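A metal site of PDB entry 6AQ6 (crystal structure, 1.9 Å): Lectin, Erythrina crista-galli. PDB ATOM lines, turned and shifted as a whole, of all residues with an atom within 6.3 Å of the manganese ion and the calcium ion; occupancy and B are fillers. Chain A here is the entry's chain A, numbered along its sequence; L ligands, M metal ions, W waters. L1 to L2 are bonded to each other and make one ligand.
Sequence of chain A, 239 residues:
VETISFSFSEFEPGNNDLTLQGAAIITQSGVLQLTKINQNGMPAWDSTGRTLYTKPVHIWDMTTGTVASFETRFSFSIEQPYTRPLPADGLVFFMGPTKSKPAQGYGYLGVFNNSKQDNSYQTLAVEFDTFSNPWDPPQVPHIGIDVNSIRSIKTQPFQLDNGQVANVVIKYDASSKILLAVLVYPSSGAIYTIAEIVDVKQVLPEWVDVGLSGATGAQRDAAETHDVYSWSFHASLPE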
ATOM      1  N   ASP A  89      12.729  11.255  21.995  1.00  0.00           N
ATOM      2  CA  ASP A  89      13.976  12.032  21.989  1.00  0.00           C
ATOM      3  C   ASP A  89      14.767  11.832  20.683  1.00  0.00           C
ATOM      4  O   ASP A  89      15.537  12.688  20.278  1.00  0.00           O
ATOM      5  CB  ASP A  89      14.896  11.624  23.165  1.00  0.00           C
ATOM      6  CG  ASP A  89      14.685  12.484  24.427  1.00  0.00           C
ATOM      7  OD1 ASP A  89      14.021  11.979  25.346  1.00  0.00           O
ATOM      8  OD2 ASP A  89      15.164  13.636  24.476  1.00  0.00           O
ATOM      9  N   GLY A 107      17.511  12.131  26.252  1.00  0.00           N
ATOM     10  CA  GLY A 107      18.369  12.884  25.366  1.00  0.00           C
ATOM     11  C   GLY A 107      19.730  12.247  25.150  1.00  0.00           C
ATOM     12  O   GLY A 107      20.488  12.746  24.305  1.00  0.00           O
ATOM     13  N   LEU A 109      19.864   9.087  24.211  1.00  0.00           N
ATOM     14  CA  LEU A 109      19.563   8.293  23.024  1.00  0.00           C
ATOM     15  C   LEU A 109      19.956   6.836  23.148  1.00  0.00           C
ATOM     16  O   LEU A 109      20.007   6.121  22.134  1.00  0.00           O
ATOM     17  CB  LEU A 109      20.227   8.914  21.783  1.00  0.00           C
ATOM     18  CG  LEU A 109      19.822  10.350  21.464  1.00  0.00           C
ATOM     19  CD1 LEU A 109      20.428  10.847  20.136  1.00  0.00           C
ATOM     20  CD2 LEU A 109      18.289  10.485  21.443  1.00  0.00           C
ATOM     21  N   GLU A 127      23.259  11.219  14.639  1.00  0.00           N
ATOM     22  CA  GLU A 127      22.018  11.242  15.397  1.00  0.00           C
ATOM     23  C   GLU A 127      20.952  11.989  14.597  1.00  0.00           C
ATOM     24  O   GLU A 127      21.265  12.880  13.799  1.00  0.00           O
ATOM     25  CB  GLU A 127      22.210  11.919  16.754  1.00  0.00           C
ATOM     26  CG  GLU A 127      22.490  13.412  16.656  1.00  0.00           C
ATOM     27  CD  GLU A 127      22.430  14.142  17.995  1.00  0.00           C
ATOM     28  OE1 GLU A 127      22.888  13.582  19.021  1.00  0.00           O
ATOM     29  OE2 GLU A 127      21.931  15.276  18.033  1.00  0.00           O
ATOM     30  N   ASP A 129      17.876  13.905  15.992  1.00  0.00           N
ATOM     31  CA  ASP A 129      17.564  14.338  17.351  1.00  0.00           C
ATOM     32  C   ASP A 129      16.288  15.161  17.296  1.00  0.00           C
ATOM     33  O   ASP A 129      16.230  16.142  16.547  1.00  0.00           O
ATOM     34  CB  ASP A 129      18.750  15.161  17.864  1.00  0.00           C
ATOM     35  CG  ASP A 129      18.690  15.459  19.354  1.00  0.00           C
ATOM     36  OD1 ASP A 129      17.577  15.381  19.898  1.00  0.00           O
ATOM     37  OD2 ASP A 129      19.775  15.773  19.971  1.00  0.00           O
ATOM     38  N   THR A 130      15.267  14.768  18.069  1.00  0.00           N
ATOM     39  CA  THR A 130      13.943  15.378  18.000  1.00  0.00           C
ATOM     40  C   THR A 130      13.585  16.274  19.183  1.00  0.00           C
ATOM     41  O   THR A 130      12.507  16.883  19.165  1.00  0.00           O
ATOM     42  CB  THR A 130      12.867  14.290  17.871  1.00  0.00           C
ATOM     43  OG1 THR A 130      12.973  13.370  18.966  1.00  0.00           O
ATOM     44  CG2 THR A 130      13.000  13.544  16.534  1.00  0.00           C
ATOM     45  N   PHE A 131      14.438  16.369  20.210  1.00  0.00           N
ATOM     46  CA  PHE A 131      14.142  17.201  21.380  1.00  0.00           C
ATOM     47  C   PHE A 131      15.374  18.022  21.739  1.00  0.00           C
ATOM     48  O   PHE A 131      16.477  17.476  21.832  1.00  0.00           O
ATOM     49  CB  PHE A 131      13.697  16.330  22.567  1.00  0.00           C
ATOM     50  CG  PHE A 131      13.438  17.111  23.831  1.00  0.00           C
ATOM     51  CD1 PHE A 131      12.190  17.634  24.090  1.00  0.00           C
ATOM     52  CD2 PHE A 131      14.449  17.304  24.767  1.00  0.00           C
ATOM     53  CE1 PHE A 131      11.936  18.367  25.249  1.00  0.00           C
ATOM     54  CE2 PHE A 131      14.208  18.026  25.940  1.00  0.00           C
ATOM     55  CZ  PHE A 131      12.949  18.560  26.175  1.00  0.00           C
ATOM     56  N   SER A 132      15.192  19.320  21.953  1.00  0.00           N
ATOM     57  CA  SER A 132      16.312  20.236  22.195  1.00  0.00           C
ATOM     58  C   SER A 132      16.680  20.277  23.681  1.00  0.00           C
ATOM     59  O   SER A 132      16.085  21.027  24.462  1.00  0.00           O
ATOM     60  CB  SER A 132      15.981  21.630  21.678  1.00  0.00           C
ATOM     61  OG  SER A 132      17.081  22.520  21.817  1.00  0.00           O
ATOM     62  N   ASN A 133      17.695  19.486  24.061  1.00  0.00           N
ATOM     63  CA  ASN A 133      18.245  19.462  25.414  1.00  0.00           C
ATOM     64  C   ASN A 133      19.126  20.685  25.652  1.00  0.00           C
ATOM     65  O   ASN A 133      19.429  21.427  24.718  1.00  0.00           O
ATOM     66  CB  ASN A 133      19.074  18.184  25.628  1.00  0.00           C
ATOM     67  CG  ASN A 133      18.242  16.916  25.531  1.00  0.00           C
ATOM     68  OD1 ASN A 133      18.131  16.307  24.467  1.00  0.00           O
ATOM     69  ND2 ASN A 133      17.684  16.481  26.667  1.00  0.00           N
ATOM     70  N   TRP A 135      22.251  20.853  25.868  1.00  0.00           N
ATOM     71  CA  TRP A 135      23.476  20.774  25.092  1.00  0.00           C
ATOM     72  C   TRP A 135      23.248  20.836  23.583  1.00  0.00           C
ATOM     73  O   TRP A 135      24.229  20.866  22.836  1.00  0.00           O
ATOM     74  CB  TRP A 135      24.211  19.466  25.399  1.00  0.00           C
ATOM     75  CG  TRP A 135      23.298  18.256  25.288  1.00  0.00           C
ATOM     76  CD1 TRP A 135      22.932  17.600  24.148  1.00  0.00           C
ATOM     77  CD2 TRP A 135      22.646  17.571  26.372  1.00  0.00           C
ATOM     78  NE1 TRP A 135      22.097  16.558  24.449  1.00  0.00           N
ATOM     79  CE2 TRP A 135      21.904  16.517  25.807  1.00  0.00           C
ATOM     80  CE3 TRP A 135      22.609  17.766  27.749  1.00  0.00           C
ATOM     81  CZ2 TRP A 135      21.137  15.651  26.571  1.00  0.00           C
ATOM     82  CZ3 TRP A 135      21.855  16.903  28.518  1.00  0.00           C
ATOM     83  CH2 TRP A 135      21.133  15.854  27.939  1.00  0.00           C
ATOM     84  N   ASP A 136      21.963  20.819  23.133  1.00  0.00           N
ATOM     85  CA  ASP A 136      21.479  20.802  21.758  1.00  0.00           C
ATOM     86  C   ASP A 136      21.350  22.215  21.203  1.00  0.00           C
ATOM     87  O   ASP A 136      21.123  23.169  21.957  1.00  0.00           O
ATOM     88  CB  ASP A 136      20.121  20.109  21.699  1.00  0.00           C
ATOM     89  CG  ASP A 136      20.252  18.623  21.682  1.00  0.00           C
ATOM     90  OD1 ASP A 136      21.270  18.208  21.097  1.00  0.00           O
ATOM     91  OD2 ASP A 136      19.395  17.890  22.252  1.00  0.00           O
ATOM     92  N   PRO A 137      21.493  22.399  19.887  1.00  0.00           N
ATOM     93  CA  PRO A 137      21.076  23.662  19.282  1.00  0.00           C
ATOM     94  C   PRO A 137      19.584  23.850  19.499  1.00  0.00           C
ATOM     95  O   PRO A 137      18.908  22.879  19.888  1.00  0.00           O
ATOM     96  CB  PRO A 137      21.406  23.477  17.792  1.00  0.00           C
ATOM     97  CG  PRO A 137      21.337  21.998  17.582  1.00  0.00           C
ATOM     98  CD  PRO A 137      21.870  21.399  18.874  1.00  0.00           C
ATOM     99  N   VAL A 140      15.014  21.719  16.369  1.00  0.00           N
ATOM    100  CA  VAL A 140      14.769  20.282  16.229  1.00  0.00           C
ATOM    101  C   VAL A 140      13.726  20.094  15.135  1.00  0.00           C
ATOM    102  O   VAL A 140      12.840  20.946  14.959  1.00  0.00           O
ATOM    103  CB  VAL A 140      14.327  19.654  17.554  1.00  0.00           C
ATOM    104  CG1 VAL A 140      15.525  19.474  18.495  1.00  0.00           C
ATOM    105  CG2 VAL A 140      13.211  20.486  18.197  1.00  0.00           C
ATOM    106  N   HIS A 142      17.272  17.745  14.196  1.00  0.00           N
ATOM    107  CA  HIS A 142      18.543  18.068  13.567  1.00  0.00           C
ATOM    108  C   HIS A 142      19.356  16.782  13.428  1.00  0.00           C
ATOM    109  O   HIS A 142      19.251  15.869  14.252  1.00  0.00           O
ATOM    110  CB  HIS A 142      19.332  19.118  14.359  1.00  0.00           C
ATOM    111  CG  HIS A 142      19.570  18.754  15.805  1.00  0.00           C
ATOM    112  ND1 HIS A 142      18.928  19.393  16.841  1.00  0.00           N
ATOM    113  CD2 HIS A 142      20.379  17.834  16.375  1.00  0.00           C
ATOM    114  CE1 HIS A 142      19.325  18.874  17.986  1.00  0.00           C
ATOM    115  NE2 HIS A 142      20.202  17.922  17.733  1.00  0.00           N
ATOM    116  N   GLY A 144      23.047  15.304  13.743  1.00  0.00           N
ATOM    117  CA  GLY A 144      24.264  15.646  14.448  1.00  0.00           C
ATOM    118  C   GLY A 144      25.311  14.562  14.246  1.00  0.00           C
ATOM    119  O   GLY A 144      25.008  13.364  14.202  1.00  0.00           O
ATOM    120  N   ASP A 146      28.223  12.983  16.229  1.00  0.00           N
ATOM    121  CA  ASP A 146      28.581  12.872  17.652  1.00  0.00           C
ATOM    122  C   ASP A 146      29.896  12.099  17.753  1.00  0.00           C
ATOM    123  O   ASP A 146      29.943  10.904  17.435  1.00  0.00           O
ATOM    124  CB  ASP A 146      27.496  12.153  18.442  1.00  0.00           C
ATOM    125  CG  ASP A 146      26.130  12.862  18.385  1.00  0.00           C
ATOM    126  OD1 ASP A 146      26.058  14.001  17.901  1.00  0.00           O
ATOM    127  OD2 ASP A 146      25.137  12.247  18.841  1.00  0.00           O
ATOM    128  N   ILE A 150      27.383  13.193  23.289  1.00  0.00           N
ATOM    129  CA  ILE A 150      26.065  13.575  22.770  1.00  0.00           C
ATOM    130  C   ILE A 150      26.045  15.024  22.317  1.00  0.00           C
ATOM    131  O   ILE A 150      25.118  15.439  21.602  1.00  0.00           O
ATOM    132  CB  ILE A 150      25.004  13.298  23.851  1.00  0.00           C
ATOM    133  CG1 ILE A 150      23.587  13.383  23.244  1.00  0.00           C
ATOM    134  CG2 ILE A 150      25.193  14.280  25.019  1.00  0.00           C
ATOM    135  CD1 ILE A 150      23.219  12.181  22.355  1.00  0.00           C
ATOM    136  N   SER A 152      27.093  17.311  19.805  1.00  0.00           N
ATOM    137  CA  SER A 152      27.583  17.105  18.452  1.00  0.00           C
ATOM    138  C   SER A 152      28.637  18.139  18.086  1.00  0.00           C
ATOM    139  O   SER A 152      28.528  19.331  18.404  1.00  0.00           O
ATOM    140  CB  SER A 152      26.406  17.193  17.462  1.00  0.00           C
ATOM    141  OG  SER A 152      25.324  16.431  17.967  1.00  0.00           O
ATOM    142  N   THR A 155      25.989  20.115  13.602  1.00  0.00           N
ATOM    143  CA  THR A 155      24.557  19.856  13.515  1.00  0.00           C
ATOM    144  C   THR A 155      23.964  20.499  12.268  1.00  0.00           C
ATOM    145  O   THR A 155      24.495  21.473  11.735  1.00  0.00           O
ATOM    146  CB  THR A 155      23.788  20.368  14.757  1.00  0.00           C
ATOM    147  OG1 THR A 155      23.894  21.793  14.861  1.00  0.00           O
ATOM    148  CG2 THR A 155      24.326  19.725  16.028  1.00  0.00           C
HETATM  149  C1  LIG L   1      11.950  16.773  34.546  1.00  0.00           C
HETATM  150  C2  LIG L   1      10.931  16.795  33.426  1.00  0.00           C
HETATM  151  C3  LIG L   1      11.470  15.903  32.324  1.00  0.00           C
HETATM  152  C4  LIG L   1      12.804  16.459  31.853  1.00  0.00           C
HETATM  153  C5  LIG L   1      13.729  16.859  32.990  1.00  0.00           C
HETATM  154  C6  LIG L   1      14.735  17.857  32.480  1.00  0.00           C
HETATM  155  C7  LIG L   1       8.555  17.169  33.904  1.00  0.00           C
HETATM  156  C8  LIG L   1       7.233  16.647  34.402  1.00  0.00           C
HETATM  157  N1  LIG L   1       9.693  16.304  33.900  1.00  0.00           N
HETATM  158  O1  LIG L   1      11.459  17.424  35.695  1.00  0.00           O
HETATM  159  O2  LIG L   1      10.548  15.778  31.231  1.00  0.00           O
HETATM  160  O3  LIG L   1      13.459  15.469  31.082  1.00  0.00           O
HETATM  161  O4  LIG L   1      13.062  17.479  34.070  1.00  0.00           O
HETATM  162  O5  LIG L   1      15.737  18.021  33.465  1.00  0.00           O
HETATM  163  O6  LIG L   1       8.618  18.312  33.497  1.00  0.00           O
HETATM  164  C1  LG2 L   2      13.584  15.741  29.721  1.00  0.00           C
HETATM  165  C2  LG2 L   2      14.607  14.796  29.085  1.00  0.00           C
HETATM  166  C3  LG2 L   2      14.624  15.038  27.591  1.00  0.00           C
HETATM  167  C4  LG2 L   2      13.237  14.747  27.064  1.00  0.00           C
HETATM  168  C5  LG2 L   2      12.203  15.612  27.778  1.00  0.00           C
HETATM  169  C6  LG2 L   2      10.796  15.203  27.366  1.00  0.00           C
HETATM  170  O1  LG2 L   2      15.912  15.034  29.582  1.00  0.00           O
HETATM  171  O2  LG2 L   2      15.644  14.277  26.962  1.00  0.00           O
HETATM  172  O3  LG2 L   2      12.959  13.394  27.307  1.00  0.00           O
HETATM  173  O4  LG2 L   2      12.284  15.510  29.183  1.00  0.00           O
HETATM  174  O5  LG2 L   2       9.819  15.916  28.114  1.00  0.00           O
HETATM  175 MN    MN M   1      21.408  16.810  19.366  1.00  0.00          MN
HETATM  176 CA    CA M   2      18.295  16.043  22.084  1.00  0.00          CA
HETATM  177  O   HOH W   1      20.424  14.666  22.717  1.00  0.00           O
HETATM  178  O   HOH W   2      22.610  15.181  20.850  1.00  0.00           O
HETATM  179  O   HOH W   3      16.935  14.319  22.562  1.00  0.00           O
HETATM  180  O   HOH W   4      23.468  17.775  19.027  1.00  0.00           O
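The calcium ion is bound by the side-chain carboxylate (OD2) of Asp 136 (2.2 Å), water W3 (2.2 Å), the backbone carbonyl oxygen (O) of Phe 131 (2.3 Å), the side-chain carboxylate (OD1) of Asp 129 (2.4 Å), the side-chain amide oxygen (OD1) of Asn 133 (2.4 Å), the side-chain carboxylate (OD2) of Asp 129 (2.6 Å) and water W1 (2.6 Å).
Water W2 lies within hydrogen-bond range of OE1 of Glu 127 (2.4 Å) and O of Ile 150 (2.6 Å). Water W1 bridges the backbone carbonyl oxygen of Gly 107 (2.5 Å) and the indole nitrogen of Trp 135 (3.1 Å).
Four residues have an atom within 4 Å of the manganese ion: Glu 127, Asp 129, Asp 136 and His 142.
The nearest printed residue that does not touch the calcium ion is Trp 135 (4.5 Å).
The manganese ion is bound by the side-chain carboxylate (OD2) of Asp 129 (2.0 Å), the side-chain carboxylate (OE2) of Glu 127 (2.1 Å), the side-chain carboxylate (OD1) of Asp 136 (2.2 Å), water W4 (2.3 Å), a ring nitrogen (NE2) of His 142 (2.3 Å) and water W2 (2.5 Å).
O2 of LG2 L2 sits at hydrogen-bond distance from ND2 of Asn 133 (3.0 Å). The side-chain carboxylate (OD2) of Asp 89 is in hydrogen-bond range of an oxygen (O2) of LG2 L2, 2.6 Å away. The backbone NH of Gly 107 sits at hydrogen-bond distance from an oxygen (O2) of LG2 L2 (2.9 Å).
The backbone NH (N) of Glu 127 is in hydrogen-bond range of the backbone carbonyl oxygen (O) of Gly 144, at 2.8 Å. The side-chain carboxylate of Asp 146 lies close to the side-chain carboxylate of Glu 127 (2.6 Å).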
